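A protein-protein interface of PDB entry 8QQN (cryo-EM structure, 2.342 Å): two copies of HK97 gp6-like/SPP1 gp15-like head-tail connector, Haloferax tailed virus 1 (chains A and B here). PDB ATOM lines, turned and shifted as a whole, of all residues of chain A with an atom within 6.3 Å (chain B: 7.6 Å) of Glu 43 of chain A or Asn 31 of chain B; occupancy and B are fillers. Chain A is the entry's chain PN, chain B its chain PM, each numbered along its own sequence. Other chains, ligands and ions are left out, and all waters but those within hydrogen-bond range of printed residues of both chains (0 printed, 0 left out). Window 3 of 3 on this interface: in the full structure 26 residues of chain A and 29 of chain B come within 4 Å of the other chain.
OE2 of Glu 47 of chain A is in hydrogen-bond range of NE2 of Gln 28 of chain B, at 3.0 Å.
The guanidinium group of Arg 44 of chain A sits at hydrogen-bond distance from the backbone carbonyl oxygen of Glu 30 of chain B.
The side-chain amide nitrogen of Asn 31 of chain B lies within hydrogen-bond range of the side-chain carboxylate of Glu 47 of chain A, at 2.9 Å.
NE of Arg 44 of chain A lies within hydrogen-bond range of O of Ser 33 of chain B, at 2.7 Å.
N of Ser 34 of chain B sits at hydrogen-bond distance from O of Phe 89 of chain A (2.9 Å).
The side-chain hydroxyl (OH) of Tyr 76 of chain B is in hydrogen-bond range of the side-chain carboxylate (OE2) of Glu 47 of chain A (2.5 Å).
OD1 of Asn 31 of chain B sits close to O of Ser 27 of chain B, at 3.5 Å.
O of Leu 32 of chain B is in hydrogen-bond range of OH of Tyr 121 of chain B (2.7 Å).
OG of Ser 33 of chain B lies within hydrogen-bond range of OG1 of Thr 35 of chain B (3.0 Å).
OG of Ser 41 of chain A lies within hydrogen-bond range of OE1 of Glu 43 of chain A, at 2.6 Å.
The guanidinium group (NH2) of Arg 44 of chain A sits at hydrogen-bond distance from the side-chain hydroxyl (OG) of Ser 41 of chain A, at 3.1 Å.
CB of Glu 43 of chain A touches OD1 of Asn 31 of chain B (3.8 Å).
Arg 44 of chain A touches Asn 31 of chain B.
Arg 44 of chain A touches Ser 34 of chain B.
Arg 44 of chain A touches Gly 36 of chain B (NH1 to CA, 3.6 Å).
CD2 of Leu 32 of chain B touches CG of Glu 47 of chain A (3.9 Å).
Asn 31 of chain B touches Phe 89 of chain A.
Leu 32 of chain B touches Phe 89 of chain A (O to CD1, 3.2 Å).
Phe 89 of chain A touches Ser 33 of chain B (O to CA, 3.7 Å).
Of the printed residues of chain B, Glu 43 of chain A touches Asn 31.
Printed residues of chain B within 4 Å of Phe 89 of chain A: Asn 31, Leu 32, Ser 33 and Ser 34.
Asp 24 of chain B touches none of the printed residues of chain A.
Of chain A, only Glu 43 (3.8 Å), Arg 44 (3.4 Å), Glu 47 (2.9 Å) and Phe 89 (3.6 Å) come within 4 Å of Asn 31 of chain B.
Of the printed residues of chain A, Ser 34 of chain B touches Arg 44 (3.8 Å) and Phe 89 (2.9 Å).
Printed residues of chain A within 4 Å of Gly 36 of chain B: Arg 44 (3.6 Å).
Printed residues of chain A within 4 Å of Tyr 76 of chain B: Glu 47 (2.5 Å).
The nearest residue of chain B that does not touch Glu 43 of chain A is Ser 27 of chain B (7.0 Å).
The nearest residue of chain A that does not touch Asn 31 of chain B is Ser 41 of chain A (5.9 Å).
The nearest printed residue of chain A that does not touch Gly 36 of chain B is Phe 89 of chain A (6.8 Å).
Of the 16 printed residues of chain B, 8 touch a printed residue of chain A.
Hydrophobic or aromatic side chains of chain B that line the printed part of chain A: Leu 32 and Tyr 76.
No position is printed for both chains.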
ATOM      1  N   SER A  41     -22.201 -26.937 -14.059  1.00  0.00           N
ATOM      2  CA  SER A  41     -23.641 -26.976 -13.827  1.00  0.00           C
ATOM      3  C   SER A  41     -24.361 -28.000 -14.718  1.00  0.00           C
ATOM      4  O   SER A  41     -23.829 -28.455 -15.730  1.00  0.00           O
ATOM      5  CB  SER A  41     -24.240 -25.594 -13.943  1.00  0.00           C
ATOM      6  OG  SER A  41     -24.312 -25.168 -15.299  1.00  0.00           O
ATOM      7  N   ARG A  42     -25.605 -28.345 -14.353  1.00  0.00           N
ATOM      8  CA  ARG A  42     -26.407 -29.325 -15.074  1.00  0.00           C
ATOM      9  C   ARG A  42     -26.609 -28.950 -16.544  1.00  0.00           C
ATOM     10  O   ARG A  42     -26.481 -29.820 -17.402  1.00  0.00           O
ATOM     11  CB  ARG A  42     -27.750 -29.548 -14.377  1.00  0.00           C
ATOM     12  CG  ARG A  42     -28.539 -30.696 -14.982  1.00  0.00           C
ATOM     13  CD  ARG A  42     -30.029 -30.609 -14.707  1.00  0.00           C
ATOM     14  NE  ARG A  42     -30.708 -31.740 -15.299  1.00  0.00           N
ATOM     15  CZ  ARG A  42     -31.193 -31.802 -16.533  1.00  0.00           C
ATOM     16  NH1 ARG A  42     -31.759 -32.924 -16.919  1.00  0.00           N
ATOM     17  NH2 ARG A  42     -31.121 -30.788 -17.378  1.00  0.00           N
ATOM     18  N   GLU A  43     -26.903 -27.673 -16.837  1.00  0.00           N
ATOM     19  CA  GLU A  43     -27.198 -27.203 -18.190  1.00  0.00           C
ATOM     20  C   GLU A  43     -26.047 -27.491 -19.158  1.00  0.00           C
ATOM     21  O   GLU A  43     -26.270 -27.851 -20.312  1.00  0.00           O
ATOM     22  CB  GLU A  43     -27.488 -25.700 -18.237  1.00  0.00           C
ATOM     23  CG  GLU A  43     -28.538 -25.220 -17.249  1.00  0.00           C
ATOM     24  CD  GLU A  43     -27.967 -24.702 -15.939  1.00  0.00           C
ATOM     25  OE1 GLU A  43     -26.917 -25.217 -15.510  1.00  0.00           O
ATOM     26  OE2 GLU A  43     -28.572 -23.779 -15.353  1.00  0.00           O
ATOM     27  N   ARG A  44     -24.813 -27.353 -18.672  1.00  0.00           N
ATOM     28  CA  ARG A  44     -23.603 -27.567 -19.449  1.00  0.00           C
ATOM     29  C   ARG A  44     -23.404 -29.046 -19.765  1.00  0.00           C
ATOM     30  O   ARG A  44     -23.091 -29.392 -20.900  1.00  0.00           O
ATOM     31  CB  ARG A  44     -22.432 -26.932 -18.709  1.00  0.00           C
ATOM     32  CG  ARG A  44     -22.676 -25.445 -18.552  1.00  0.00           C
ATOM     33  CD  ARG A  44     -21.557 -24.618 -17.976  1.00  0.00           C
ATOM     34  NE  ARG A  44     -21.739 -23.226 -18.363  1.00  0.00           N
ATOM     35  CZ  ARG A  44     -22.509 -22.331 -17.749  1.00  0.00           C
ATOM     36  NH1 ARG A  44     -22.571 -21.104 -18.231  1.00  0.00           N
ATOM     37  NH2 ARG A  44     -23.204 -22.644 -16.669  1.00  0.00           N
ATOM     38  N   LYS A  45     -23.672 -29.920 -18.791  1.00  0.00           N
ATOM     39  CA  LYS A  45     -23.653 -31.362 -18.983  1.00  0.00           C
ATOM     40  C   LYS A  45     -24.757 -31.826 -19.931  1.00  0.00           C
ATOM     41  O   LYS A  45     -24.485 -32.615 -20.833  1.00  0.00           O
ATOM     42  CB  LYS A  45     -23.613 -32.063 -17.627  1.00  0.00           C
ATOM     43  CG  LYS A  45     -22.241 -31.933 -16.990  1.00  0.00           C
ATOM     44  CD  LYS A  45     -22.080 -32.586 -15.634  1.00  0.00           C
ATOM     45  CE  LYS A  45     -22.537 -31.705 -14.493  1.00  0.00           C
ATOM     46  NZ  LYS A  45     -21.952 -32.118 -13.195  1.00  0.00           N
ATOM     47  N   ALA A  46     -25.970 -31.276 -19.790  1.00  0.00           N
ATOM     48  CA  ALA A  46     -27.079 -31.547 -20.697  1.00  0.00           C
ATOM     49  C   ALA A  46     -26.758 -31.098 -22.130  1.00  0.00           C
ATOM     50  O   ALA A  46     -27.008 -31.846 -23.077  1.00  0.00           O
ATOM     51  CB  ALA A  46     -28.332 -30.909 -20.152  1.00  0.00           C
ATOM     52  N   GLU A  47     -26.161 -29.907 -22.294  1.00  0.00           N
ATOM     53  CA  GLU A  47     -25.763 -29.363 -23.588  1.00  0.00           C
ATOM     54  C   GLU A  47     -24.728 -30.259 -24.274  1.00  0.00           C
ATOM     55  O   GLU A  47     -24.849 -30.540 -25.466  1.00  0.00           O
ATOM     56  CB  GLU A  47     -25.212 -27.947 -23.434  1.00  0.00           C
ATOM     57  CG  GLU A  47     -25.193 -27.167 -24.737  1.00  0.00           C
ATOM     58  CD  GLU A  47     -26.558 -26.654 -25.167  1.00  0.00           C
ATOM     59  OE1 GLU A  47     -27.227 -25.997 -24.343  1.00  0.00           O
ATOM     60  OE2 GLU A  47     -26.955 -26.924 -26.317  1.00  0.00           O
ATOM     61  N   ALA A  48     -23.732 -30.733 -23.516  1.00  0.00           N
ATOM     62  CA  ALA A  48     -22.704 -31.648 -23.996  1.00  0.00           C
ATOM     63  C   ALA A  48     -23.295 -32.970 -24.502  1.00  0.00           C
ATOM     64  O   ALA A  48     -22.889 -33.449 -25.559  1.00  0.00           O
ATOM     65  CB  ALA A  48     -21.696 -31.883 -22.905  1.00  0.00           C
ATOM     66  N   PHE A  89     -15.367 -28.116 -22.344  1.00  0.00           N
ATOM     67  CA  PHE A  89     -16.054 -26.999 -21.702  1.00  0.00           C
ATOM     68  C   PHE A  89     -15.342 -26.539 -20.419  1.00  0.00           C
ATOM     69  O   PHE A  89     -15.454 -25.371 -20.038  1.00  0.00           O
ATOM     70  CB  PHE A  89     -17.520 -27.351 -21.416  1.00  0.00           C
ATOM     71  CG  PHE A  89     -18.430 -27.743 -22.567  1.00  0.00           C
ATOM     72  CD1 PHE A  89     -18.010 -27.766 -23.895  1.00  0.00           C
ATOM     73  CD2 PHE A  89     -19.762 -28.053 -22.310  1.00  0.00           C
ATOM     74  CE1 PHE A  89     -18.881 -28.130 -24.920  1.00  0.00           C
ATOM     75  CE2 PHE A  89     -20.634 -28.407 -23.331  1.00  0.00           C
ATOM     76  CZ  PHE A  89     -20.191 -28.459 -24.635  1.00  0.00           C
ATOM     77  N   ASP B  24     -31.983 -16.090 -25.302  1.00  0.00           N
ATOM     78  CA  ASP B  24     -32.092 -17.543 -25.274  1.00  0.00           C
ATOM     79  C   ASP B  24     -30.943 -18.212 -26.040  1.00  0.00           C
ATOM     80  O   ASP B  24     -30.350 -19.178 -25.553  1.00  0.00           O
ATOM     81  CB  ASP B  24     -33.441 -17.997 -25.835  1.00  0.00           C
ATOM     82  CG  ASP B  24     -34.673 -17.604 -25.030  1.00  0.00           C
ATOM     83  OD1 ASP B  24     -34.531 -17.159 -23.863  1.00  0.00           O
ATOM     84  OD2 ASP B  24     -35.789 -17.782 -25.568  1.00  0.00           O
ATOM     85  N   ILE B  25     -30.613 -17.699 -27.233  1.00  0.00           N
ATOM     86  CA  ILE B  25     -29.492 -18.196 -28.024  1.00  0.00           C
ATOM     87  C   ILE B  25     -28.159 -17.888 -27.328  1.00  0.00           C
ATOM     88  O   ILE B  25     -27.293 -18.756 -27.264  1.00  0.00           O
ATOM     89  CB  ILE B  25     -29.558 -17.688 -29.481  1.00  0.00           C
ATOM     90  CG1 ILE B  25     -30.801 -18.218 -30.201  1.00  0.00           C
ATOM     91  CG2 ILE B  25     -28.286 -18.048 -30.246  1.00  0.00           C
ATOM     92  CD1 ILE B  25     -31.090 -17.545 -31.534  1.00  0.00           C
ATOM     93  N   ILE B  26     -28.003 -16.675 -26.776  1.00  0.00           N
ATOM     94  CA  ILE B  26     -26.817 -16.284 -26.019  1.00  0.00           C
ATOM     95  C   ILE B  26     -26.614 -17.234 -24.836  1.00  0.00           C
ATOM     96  O   ILE B  26     -25.505 -17.719 -24.626  1.00  0.00           O
ATOM     97  CB  ILE B  26     -26.866 -14.795 -25.597  1.00  0.00           C
ATOM     98  CG1 ILE B  26     -26.712 -13.868 -26.805  1.00  0.00           C
ATOM     99  CG2 ILE B  26     -25.801 -14.481 -24.547  1.00  0.00           C
ATOM    100  CD1 ILE B  26     -27.266 -12.476 -26.600  1.00  0.00           C
ATOM    101  N   SER B  27     -27.697 -17.539 -24.109  1.00  0.00           N
ATOM    102  CA  SER B  27     -27.709 -18.471 -22.991  1.00  0.00           C
ATOM    103  C   SER B  27     -27.249 -19.868 -23.424  1.00  0.00           C
ATOM    104  O   SER B  27     -26.416 -20.483 -22.754  1.00  0.00           O
ATOM    105  CB  SER B  27     -29.071 -18.478 -22.354  1.00  0.00           C
ATOM    106  OG  SER B  27     -29.110 -19.364 -21.251  1.00  0.00           O
ATOM    107  N   GLN B  28     -27.728 -20.350 -24.579  1.00  0.00           N
ATOM    108  CA  GLN B  28     -27.283 -21.622 -25.137  1.00  0.00           C
ATOM    109  C   GLN B  28     -25.778 -21.625 -25.455  1.00  0.00           C
ATOM    110  O   GLN B  28     -25.082 -22.592 -25.143  1.00  0.00           O
ATOM    111  CB  GLN B  28     -28.132 -22.019 -26.344  1.00  0.00           C
ATOM    112  CG  GLN B  28     -27.855 -23.456 -26.767  1.00  0.00           C
ATOM    113  CD  GLN B  28     -28.663 -23.978 -27.929  1.00  0.00           C
ATOM    114  OE1 GLN B  28     -29.261 -23.214 -28.684  1.00  0.00           O
ATOM    115  NE2 GLN B  28     -28.655 -25.300 -28.099  1.00  0.00           N
ATOM    116  N   VAL B  29     -25.250 -20.551 -26.053  1.00  0.00           N
ATOM    117  CA  VAL B  29     -23.819 -20.439 -26.326  1.00  0.00           C
ATOM    118  C   VAL B  29     -23.004 -20.458 -25.029  1.00  0.00           C
ATOM    119  O   VAL B  29     -21.982 -21.140 -24.962  1.00  0.00           O
ATOM    120  CB  VAL B  29     -23.493 -19.218 -27.210  1.00  0.00           C
ATOM    121  CG1 VAL B  29     -21.994 -18.994 -27.351  1.00  0.00           C
ATOM    122  CG2 VAL B  29     -24.088 -19.386 -28.592  1.00  0.00           C
ATOM    123  N   GLU B  30     -23.473 -19.763 -23.985  1.00  0.00           N
ATOM    124  CA  GLU B  30     -22.817 -19.734 -22.684  1.00  0.00           C
ATOM    125  C   GLU B  30     -22.739 -21.111 -22.012  1.00  0.00           C
ATOM    126  O   GLU B  30     -21.922 -21.294 -21.113  1.00  0.00           O
ATOM    127  CB  GLU B  30     -23.501 -18.733 -21.760  1.00  0.00           C
ATOM    128  CG  GLU B  30     -23.276 -17.286 -22.144  1.00  0.00           C
ATOM    129  CD  GLU B  30     -23.977 -16.296 -21.228  1.00  0.00           C
ATOM    130  OE1 GLU B  30     -24.955 -16.687 -20.556  1.00  0.00           O
ATOM    131  OE2 GLU B  30     -23.539 -15.132 -21.173  1.00  0.00           O
ATOM    132  N   ASN B  31     -23.554 -22.088 -22.432  1.00  0.00           N
ATOM    133  CA  ASN B  31     -23.454 -23.449 -21.919  1.00  0.00           C
ATOM    134  C   ASN B  31     -22.189 -24.172 -22.400  1.00  0.00           C
ATOM    135  O   ASN B  31     -21.817 -25.186 -21.811  1.00  0.00           O
ATOM    136  CB  ASN B  31     -24.695 -24.280 -22.256  1.00  0.00           C
ATOM    137  CG  ASN B  31     -25.959 -23.818 -21.560  1.00  0.00           C
ATOM    138  OD1 ASN B  31     -25.903 -23.120 -20.549  1.00  0.00           O
ATOM    139  ND2 ASN B  31     -27.103 -24.224 -22.088  1.00  0.00           N
ATOM    140  N   LEU B  32     -21.518 -23.669 -23.445  1.00  0.00           N
ATOM    141  CA  LEU B  32     -20.349 -24.335 -24.013  1.00  0.00           C
ATOM    142  C   LEU B  32     -19.044 -24.017 -23.269  1.00  0.00           C
ATOM    143  O   LEU B  32     -18.001 -24.583 -23.589  1.00  0.00           O
ATOM    144  CB  LEU B  32     -20.244 -24.018 -25.508  1.00  0.00           C
ATOM    145  CG  LEU B  32     -21.446 -24.404 -26.369  1.00  0.00           C
ATOM    146  CD1 LEU B  32     -21.147 -24.113 -27.826  1.00  0.00           C
ATOM    147  CD2 LEU B  32     -21.826 -25.866 -26.207  1.00  0.00           C
ATOM    148  N   SER B  33     -19.073 -23.121 -22.275  1.00  0.00           N
ATOM    149  CA  SER B  33     -17.946 -22.952 -21.371  1.00  0.00           C
ATOM    150  C   SER B  33     -18.429 -23.039 -19.929  1.00  0.00           C
ATOM    151  O   SER B  33     -19.453 -22.450 -19.589  1.00  0.00           O
ATOM    152  CB  SER B  33     -17.246 -21.650 -21.612  1.00  0.00           C
ATOM    153  OG  SER B  33     -16.210 -21.489 -20.656  1.00  0.00           O
ATOM    154  N   SER B  34     -17.650 -23.720 -19.080  1.00  0.00           N
ATOM    155  CA  SER B  34     -17.898 -23.806 -17.646  1.00  0.00           C
ATOM    156  C   SER B  34     -17.863 -22.433 -16.963  1.00  0.00           C
ATOM    157  O   SER B  34     -18.523 -22.240 -15.941  1.00  0.00           O
ATOM    158  CB  SER B  34     -16.937 -24.765 -16.995  1.00  0.00           C
ATOM    159  OG  SER B  34     -15.604 -24.366 -17.270  1.00  0.00           O
ATOM    160  N   THR B  35     -17.095 -21.483 -17.515  1.00  0.00           N
ATOM    161  CA  THR B  35     -17.058 -20.111 -17.015  1.00  0.00           C
ATOM    162  C   THR B  35     -18.224 -19.270 -17.541  1.00  0.00           C
ATOM    163  O   THR B  35     -18.521 -18.224 -16.969  1.00  0.00           O
ATOM    164  CB  THR B  35     -15.727 -19.421 -17.347  1.00  0.00           C
ATOM    165  OG1 THR B  35     -15.604 -19.242 -18.757  1.00  0.00           O
ATOM    166  CG2 THR B  35     -14.524 -20.191 -16.848  1.00  0.00           C
ATOM    167  N   GLY B  36     -18.850 -19.687 -18.652  1.00  0.00           N
ATOM    168  CA  GLY B  36     -19.931 -18.961 -19.306  1.00  0.00           C
ATOM    169  C   GLY B  36     -19.527 -17.601 -19.880  1.00  0.00           C
ATOM    170  O   GLY B  36     -20.407 -16.845 -20.287  1.00  0.00           O
ATOM    171  N   TRP B  37     -18.217 -17.291 -19.902  1.00  0.00           N
ATOM    172  CA  TRP B  37     -17.670 -15.976 -20.233  1.00  0.00           C
ATOM    173  C   TRP B  37     -18.452 -14.848 -19.546  1.00  0.00           C
ATOM    174  O   TRP B  37     -18.824 -13.863 -20.186  1.00  0.00           O
ATOM    175  CB  TRP B  37     -17.567 -15.776 -21.758  1.00  0.00           C
ATOM    176  CG  TRP B  37     -16.868 -16.878 -22.495  1.00  0.00           C
ATOM    177  CD1 TRP B  37     -15.520 -17.063 -22.605  1.00  0.00           C
ATOM    178  CD2 TRP B  37     -17.480 -17.949 -23.253  1.00  0.00           C
ATOM    179  NE1 TRP B  37     -15.258 -18.173 -23.368  1.00  0.00           N
ATOM    180  CE2 TRP B  37     -16.436 -18.740 -23.789  1.00  0.00           C
ATOM    181  CE3 TRP B  37     -18.802 -18.323 -23.531  1.00  0.00           C
ATOM    182  CZ2 TRP B  37     -16.684 -19.877 -24.576  1.00  0.00           C
ATOM    183  CZ3 TRP B  37     -19.051 -19.440 -24.310  1.00  0.00           C
ATOM    184  CH2 TRP B  37     -18.003 -20.213 -24.821  1.00  0.00           C
ATOM    185  N   TYR B  76     -25.317 -26.981 -33.694  1.00  0.00           N
ATOM    186  CA  TYR B  76     -24.078 -27.125 -32.941  1.00  0.00           C
ATOM    187  C   TYR B  76     -22.874 -26.537 -33.664  1.00  0.00           C
ATOM    188  O   TYR B  76     -22.050 -25.912 -33.015  1.00  0.00           O
ATOM    189  CB  TYR B  76     -23.898 -28.543 -32.401  1.00  0.00           C
ATOM    190  CG  TYR B  76     -24.779 -28.717 -31.192  1.00  0.00           C
ATOM    191  CD1 TYR B  76     -24.471 -28.044 -30.021  1.00  0.00           C
ATOM    192  CD2 TYR B  76     -25.974 -29.427 -31.243  1.00  0.00           C
ATOM    193  CE1 TYR B  76     -25.302 -28.100 -28.912  1.00  0.00           C
ATOM    194  CE2 TYR B  76     -26.809 -29.505 -30.137  1.00  0.00           C
ATOM    195  CZ  TYR B  76     -26.469 -28.844 -28.966  1.00  0.00           C
ATOM    196  OH  TYR B  76     -27.287 -28.889 -27.872  1.00  0.00           O
ATOM    197  N   TYR B 121     -13.002 -25.002 -29.492  1.00  0.00           N
ATOM    198  CA  TYR B 121     -14.299 -24.838 -30.130  1.00  0.00           C
ATOM    199  C   TYR B 121     -14.185 -24.844 -31.652  1.00  0.00           C
ATOM    200  O   TYR B 121     -15.038 -25.400 -32.333  1.00  0.00           O
ATOM    201  CB  TYR B 121     -14.972 -23.570 -29.613  1.00  0.00           C
ATOM    202  CG  TYR B 121     -15.118 -23.564 -28.117  1.00  0.00           C
ATOM    203  CD1 TYR B 121     -15.970 -24.472 -27.506  1.00  0.00           C
ATOM    204  CD2 TYR B 121     -14.392 -22.695 -27.311  1.00  0.00           C
ATOM    205  CE1 TYR B 121     -16.103 -24.526 -26.130  1.00  0.00           C
ATOM    206  CE2 TYR B 121     -14.511 -22.739 -25.925  1.00  0.00           C
ATOM    207  CZ  TYR B 121     -15.375 -23.654 -25.341  1.00  0.00           C
ATOM    208  OH  TYR B 121     -15.514 -23.720 -23.988  1.00  0.00           O
